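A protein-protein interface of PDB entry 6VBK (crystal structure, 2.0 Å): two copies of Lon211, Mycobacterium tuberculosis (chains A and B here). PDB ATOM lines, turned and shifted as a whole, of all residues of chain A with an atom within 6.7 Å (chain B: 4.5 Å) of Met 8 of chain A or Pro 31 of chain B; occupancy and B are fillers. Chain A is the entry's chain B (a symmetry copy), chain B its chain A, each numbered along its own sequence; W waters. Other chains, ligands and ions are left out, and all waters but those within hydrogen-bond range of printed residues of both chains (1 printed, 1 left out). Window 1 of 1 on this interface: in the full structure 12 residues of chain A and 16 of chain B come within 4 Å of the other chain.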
ATOM      1  N   MET A   2      19.305 -34.522   0.480  1.00  0.00           N
ATOM      2  CA  MET A   2      18.456 -33.623  -0.289  1.00  0.00           C
ATOM      3  C   MET A   2      18.450 -32.241   0.347  1.00  0.00           C
ATOM      4  O   MET A   2      18.472 -32.104   1.572  1.00  0.00           O
ATOM      5  CB  MET A   2      17.029 -34.167  -0.363  1.00  0.00           C
ATOM      6  CG  MET A   2      16.712 -34.961  -1.618  1.00  0.00           C
ATOM      7  SD  MET A   2      15.086 -35.737  -1.523  1.00  0.00           S
ATOM      8  CE  MET A   2      14.074 -34.350  -1.014  1.00  0.00           C
ATOM      9  N   ASP A   3      18.423 -31.209  -0.491  1.00  0.00           N
ATOM     10  CA  ASP A   3      18.356 -29.839   0.006  1.00  0.00           C
ATOM     11  C   ASP A   3      16.914 -29.539   0.389  1.00  0.00           C
ATOM     12  O   ASP A   3      16.035 -29.460  -0.475  1.00  0.00           O
ATOM     13  CB  ASP A   3      18.871 -28.855  -1.040  1.00  0.00           C
ATOM     14  CG  ASP A   3      19.150 -27.479  -0.458  1.00  0.00           C
ATOM     15  OD1 ASP A   3      18.471 -27.083   0.513  1.00  0.00           O
ATOM     16  OD2 ASP A   3      20.053 -26.790  -0.970  1.00  0.00           O
ATOM     17  N   LEU A   4      16.668 -29.371   1.688  1.00  0.00           N
ATOM     18  CA  LEU A   4      15.334 -29.119   2.213  1.00  0.00           C
ATOM     19  C   LEU A   4      15.121 -27.654   2.576  1.00  0.00           C
ATOM     20  O   LEU A   4      14.209 -27.336   3.346  1.00  0.00           O
ATOM     21  CB  LEU A   4      15.073 -30.017   3.422  1.00  0.00           C
ATOM     22  CG  LEU A   4      15.314 -31.504   3.156  1.00  0.00           C
ATOM     23  CD1 LEU A   4      15.038 -32.333   4.400  1.00  0.00           C
ATOM     24  CD2 LEU A   4      14.467 -31.983   1.984  1.00  0.00           C
ATOM     25  N   GLU A   5      15.951 -26.758   2.038  1.00  0.00           N
ATOM     26  CA  GLU A   5      15.793 -25.322   2.233  1.00  0.00           C
ATOM     27  C   GLU A   5      15.774 -24.579   0.901  1.00  0.00           C
ATOM     28  O   GLU A   5      16.094 -23.387   0.856  1.00  0.00           O
ATOM     29  CB  GLU A   5      16.901 -24.774   3.136  1.00  0.00           C
ATOM     30  CG  GLU A   5      16.758 -25.179   4.596  1.00  0.00           C
ATOM     31  CD  GLU A   5      18.086 -25.506   5.249  1.00  0.00           C
ATOM     32  OE1 GLU A   5      19.076 -25.713   4.514  1.00  0.00           O
ATOM     33  OE2 GLU A   5      18.142 -25.561   6.496  1.00  0.00           O
ATOM     34  N   LEU A   6      15.408 -25.264  -0.181  1.00  0.00           N
ATOM     35  CA  LEU A   6      15.387 -24.645  -1.499  1.00  0.00           C
ATOM     36  C   LEU A   6      14.299 -23.584  -1.575  1.00  0.00           C
ATOM     37  O   LEU A   6      13.159 -23.814  -1.159  1.00  0.00           O
ATOM     38  CB  LEU A   6      15.157 -25.704  -2.577  1.00  0.00           C
ATOM     39  CG  LEU A   6      16.240 -26.765  -2.775  1.00  0.00           C
ATOM     40  CD1 LEU A   6      15.798 -27.782  -3.812  1.00  0.00           C
ATOM     41  CD2 LEU A   6      17.540 -26.108  -3.190  1.00  0.00           C
ATOM     42  N   SER A   7      14.652 -22.422  -2.114  1.00  0.00           N
ATOM     43  CA  SER A   7      13.675 -21.370  -2.361  1.00  0.00           C
ATOM     44  C   SER A   7      12.867 -21.726  -3.605  1.00  0.00           C
ATOM     45  O   SER A   7      13.436 -21.967  -4.674  1.00  0.00           O
ATOM     46  CB  SER A   7      14.374 -20.023  -2.530  1.00  0.00           C
ATOM     47  OG  SER A   7      13.437 -18.990  -2.781  1.00  0.00           O
ATOM     48  N   MET A   8      11.546 -21.767  -3.464  1.00  0.00           N
ATOM     49  CA  MET A   8      10.645 -22.130  -4.550  1.00  0.00           C
ATOM     50  C   MET A   8       9.759 -20.938  -4.870  1.00  0.00           C
ATOM     51  O   MET A   8       9.054 -20.430  -3.990  1.00  0.00           O
ATOM     52  CB  MET A   8       9.795 -23.346  -4.179  1.00  0.00           C
ATOM     53  CG  MET A   8       8.792 -23.761  -5.245  1.00  0.00           C
ATOM     54  SD  MET A   8       9.499 -24.832  -6.511  1.00  0.00           S
ATOM     55  CE  MET A   8       9.847 -26.304  -5.550  1.00  0.00           C
ATOM     56  N   SER A   9       9.795 -20.492  -6.120  1.00  0.00           N
ATOM     57  CA  SER A   9       8.935 -19.412  -6.572  1.00  0.00           C
ATOM     58  C   SER A   9       7.651 -19.977  -7.171  1.00  0.00           C
ATOM     59  O   SER A   9       7.603 -21.114  -7.646  1.00  0.00           O
ATOM     60  CB  SER A   9       9.659 -18.537  -7.595  1.00  0.00           C
ATOM     61  OG  SER A   9      10.793 -17.913  -7.018  1.00  0.00           O
ATOM     62  N   GLU A  10       6.604 -19.161  -7.142  1.00  0.00           N
ATOM     63  CA  GLU A  10       5.301 -19.581  -7.640  1.00  0.00           C
ATOM     64  C   GLU A  10       5.264 -19.506  -9.161  1.00  0.00           C
ATOM     65  O   GLU A  10       5.841 -18.599  -9.767  1.00  0.00           O
ATOM     66  CB  GLU A  10       4.203 -18.706  -7.036  1.00  0.00           C
ATOM     67  CG  GLU A  10       2.973 -19.472  -6.579  1.00  0.00           C
ATOM     68  CD  GLU A  10       2.031 -18.616  -5.754  1.00  0.00           C
ATOM     69  OE1 GLU A  10       2.425 -17.494  -5.375  1.00  0.00           O
ATOM     70  OE2 GLU A  10       0.898 -19.066  -5.486  1.00  0.00           O
ATOM     71  N   VAL B  30       8.488 -31.289   0.735  1.00  0.00           N
ATOM     72  CA  VAL B  30       9.847 -30.938   0.330  1.00  0.00           C
ATOM     73  C   VAL B  30       9.822 -30.445  -1.111  1.00  0.00           C
ATOM     74  O   VAL B  30       8.906 -30.766  -1.883  1.00  0.00           O
ATOM     75  CB  VAL B  30      10.818 -32.133   0.483  1.00  0.00           C
ATOM     76  CG1 VAL B  30      10.816 -32.651   1.914  1.00  0.00           C
ATOM     77  CG2 VAL B  30      10.460 -33.240  -0.490  1.00  0.00           C
ATOM     78  N   PRO B  31      10.813 -29.645  -1.497  1.00  0.00           N
ATOM     79  CA  PRO B  31      10.987 -29.296  -2.909  1.00  0.00           C
ATOM     80  C   PRO B  31      11.821 -30.337  -3.641  1.00  0.00           C
ATOM     81  O   PRO B  31      12.628 -31.060  -3.053  1.00  0.00           O
ATOM     82  CB  PRO B  31      11.730 -27.956  -2.839  1.00  0.00           C
ATOM     83  CG  PRO B  31      12.563 -28.089  -1.611  1.00  0.00           C
ATOM     84  CD  PRO B  31      11.744 -28.897  -0.631  1.00  0.00           C
ATOM     85  N   LEU B  32      11.615 -30.399  -4.955  1.00  0.00           N
ATOM     86  CA  LEU B  32      12.318 -31.349  -5.808  1.00  0.00           C
ATOM     87  C   LEU B  32      12.966 -30.603  -6.963  1.00  0.00           C
ATOM     88  O   LEU B  32      12.284 -29.892  -7.708  1.00  0.00           O
ATOM     89  CB  LEU B  32      11.370 -32.432  -6.333  1.00  0.00           C
ATOM     90  CG  LEU B  32      10.955 -33.519  -5.340  1.00  0.00           C
ATOM     91  CD1 LEU B  32      10.106 -34.574  -6.033  1.00  0.00           C
ATOM     92  CD2 LEU B  32      12.177 -34.151  -4.692  1.00  0.00           C
ATOM     93  N   ASP B  33      14.278 -30.780  -7.118  1.00  0.00           N
ATOM     94  CA  ASP B  33      15.004 -30.145  -8.249  1.00  0.00           C
ATOM     95  C   ASP B  33      14.877 -31.069  -9.463  1.00  0.00           C
ATOM     96  O   ASP B  33      15.618 -32.060  -9.521  1.00  0.00           O
ATOM     97  CB  ASP B  33      16.463 -29.858  -7.898  1.00  0.00           C
ATOM     98  CG  ASP B  33      17.216 -29.162  -9.016  1.00  0.00           C
ATOM     99  OD1 ASP B  33      16.770 -29.267 -10.170  1.00  0.00           O
ATOM    100  OD2 ASP B  33      18.233 -28.516  -8.717  1.00  0.00           O
ATOM    101  N   GLY B  89       7.059 -25.199  -9.495  1.00  0.00           N
ATOM    102  CA  GLY B  89       7.600 -23.856  -9.470  1.00  0.00           C
ATOM    103  C   GLY B  89       8.991 -23.778 -10.063  1.00  0.00           C
ATOM    104  O   GLY B  89       9.391 -24.656 -10.834  1.00  0.00           O
ATOM    105  N   ARG B  90       9.740 -22.737  -9.712  1.00  0.00           N
ATOM    106  CA  ARG B  90      11.095 -22.554 -10.211  1.00  0.00           C
ATOM    107  C   ARG B  90      12.040 -22.284  -9.052  1.00  0.00           C
ATOM    108  O   ARG B  90      11.713 -21.531  -8.130  1.00  0.00           O
ATOM    109  CB  ARG B  90      11.167 -21.410 -11.227  1.00  0.00           C
ATOM    110  CG  ARG B  90      10.430 -21.699 -12.523  1.00  0.00           C
ATOM    111  CD  ARG B  90      11.180 -22.691 -13.392  1.00  0.00           C
ATOM    112  NE  ARG B  90      10.315 -23.278 -14.410  1.00  0.00           N
ATOM    113  CZ  ARG B  90      10.754 -23.952 -15.466  1.00  0.00           C
ATOM    114  NH1 ARG B  90      12.056 -24.117 -15.653  1.00  0.00           N
ATOM    115  NH2 ARG B  90       9.892 -24.456 -16.339  1.00  0.00           N
ATOM    116  N   LEU B  91      13.205 -22.906  -9.108  1.00  0.00           N
ATOM    117  CA  LEU B  91      14.276 -22.749  -8.141  1.00  0.00           C
ATOM    118  C   LEU B  91      15.149 -21.560  -8.527  1.00  0.00           C
ATOM    119  O   LEU B  91      15.083 -21.082  -9.664  1.00  0.00           O
ATOM    120  CB  LEU B  91      15.091 -24.039  -8.072  1.00  0.00           C
ATOM    121  CG  LEU B  91      14.253 -25.291  -7.791  1.00  0.00           C
ATOM    122  CD1 LEU B  91      15.116 -26.542  -7.798  1.00  0.00           C
ATOM    123  CD2 LEU B  91      13.504 -25.158  -6.471  1.00  0.00           C
ATOM    124  N   GLY B  97      10.987 -26.940 -10.777  1.00  0.00           N
ATOM    125  CA  GLY B  97      10.837 -27.489  -9.451  1.00  0.00           C
ATOM    126  C   GLY B  97       9.416 -27.956  -9.211  1.00  0.00           C
ATOM    127  O   GLY B  97       8.475 -27.540  -9.886  1.00  0.00           O
ATOM    128  N   ALA B  98       9.280 -28.840  -8.225  1.00  0.00           N
ATOM    129  CA  ALA B  98       7.987 -29.380  -7.839  1.00  0.00           C
ATOM    130  C   ALA B  98       7.926 -29.512  -6.327  1.00  0.00           C
ATOM    131  O   ALA B  98       8.919 -29.864  -5.684  1.00  0.00           O
ATOM    132  CB  ALA B  98       7.726 -30.743  -8.496  1.00  0.00           C
ATOM    133  N   VAL B  99       6.759 -29.218  -5.766  1.00  0.00           N
ATOM    134  CA  VAL B  99       6.491 -29.415  -4.348  1.00  0.00           C
ATOM    135  C   VAL B  99       5.775 -30.749  -4.198  1.00  0.00           C
ATOM    136  O   VAL B  99       4.720 -30.968  -4.806  1.00  0.00           O
ATOM    137  CB  VAL B  99       5.650 -28.267  -3.768  1.00  0.00           C
ATOM    138  CG1 VAL B  99       5.349 -28.522  -2.300  1.00  0.00           C
ATOM    139  CG2 VAL B  99       6.370 -26.939  -3.951  1.00  0.00           C
HETATM  140  O   HOH W   1      13.436 -19.575  -6.853  1.00  0.00           O
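The backbone NH of Leu 32 of chain B sits at hydrogen-bond distance from the backbone carbonyl oxygen of Ala 98 of chain B (2.8 Å).
The backbone NH (N) of Gly 89 of chain B sits at hydrogen-bond distance from the backbone carbonyl oxygen (O) of Gly 97 of chain B, at 2.8 Å.
The side-chain carboxylate (OD1) of Asp 3 of chain A lies within hydrogen-bond range of the backbone NH (N) of Glu 5 of chain A, 3.0 Å away.
The backbone carbonyl oxygen of Arg 90 of chain B lies within hydrogen-bond range of the backbone NH of Ser 9 of chain A (3.0 Å).
No position is printed for both chains.
Of the 14 pairs that touch across the chains among the printed residues, none has its exchanged pair printed and touching as well.
Water W1 lies within hydrogen-bond range of the backbone carbonyl oxygen of Arg 90 of chain B (2.9 Å), the side-chain hydroxyl of Ser 9 of chain A (3.1 Å) and the backbone carbonyl oxygen of Ser 7 of chain A (3.2 Å).
Of the printed residues of chain B, Leu 4 of chain A touches Val 30.
Of the printed residues of chain B, Leu 6 of chain A touches Pro 31.
Printed residues of chain B within 4 Å of Met 8 of chain A: Pro 31, Gly 89, Arg 90, Leu 91, Ala 98 and Val 99.
Printed residues of chain A within 4 Å of Val 30 of chain B: Met 2 (3.8 Å) and Leu 4 (3.7 Å).
Pro 31 of chain B touches just these residues of chain A: Asp 3 (3.9 Å), Leu 6 (3.7 Å) and Met 8 (3.7 Å).
Of the printed residues of chain A, Ala 98 of chain B touches Met 8.
The nearest residue of chain A that does not touch Pro 31 of chain B is Met 2 of chain A (4.1 Å).
The nearest printed residue of chain B that does not touch Met 2 of chain A is Pro 31 of chain B (4.1 Å).
Of the 10 printed residues of chain B, 7 touch a printed residue of chain A.
Printed residues of chain B that touch a printed residue of chain A: Val 30, Pro 31, Gly 89, Arg 90, Leu 91, Ala 98 and Val 99.
Hydrophobic or aromatic side chains of chain A within 4 Å of the printed part of chain B: Met 2, Leu 4, Leu 6 and Met 8.
Among the printed residues, 14 pairs touch across the chains.
Among the printed residues, no Asp or Glu carboxylate lies within 4 Å of a Lys or Arg side-chain nitrogen of the other chain.
Val 30 of chain B touches Met 2 of chain A (CG2 to CE, 3.8 Å).
Asp 3 of chain A touches Pro 31 of chain B (O to CG, 3.9 Å).
Arg 90 of chain B touches Ser 7 of chain A.
Ser 7 of chain A touches Leu 91 of chain B (O to CA, 3.7 Å).
Met 8 of chain A touches Pro 31 of chain B (CE to CB, 3.7 Å).
CA of Gly 89 of chain B touches SD of Met 8 of chain A (3.6 Å).
CA of Met 8 of chain A touches O of Arg 90 of chain B, 3.8 Å away.
Leu 91 of chain B touches Met 8 of chain A (CD2 to CE, 3.9 Å).
Met 8 of chain A touches Ala 98 of chain B (CE to O, 3.7 Å).
O of Ser 9 of chain A touches CA of Gly 89 of chain B, at 3.3 Å.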
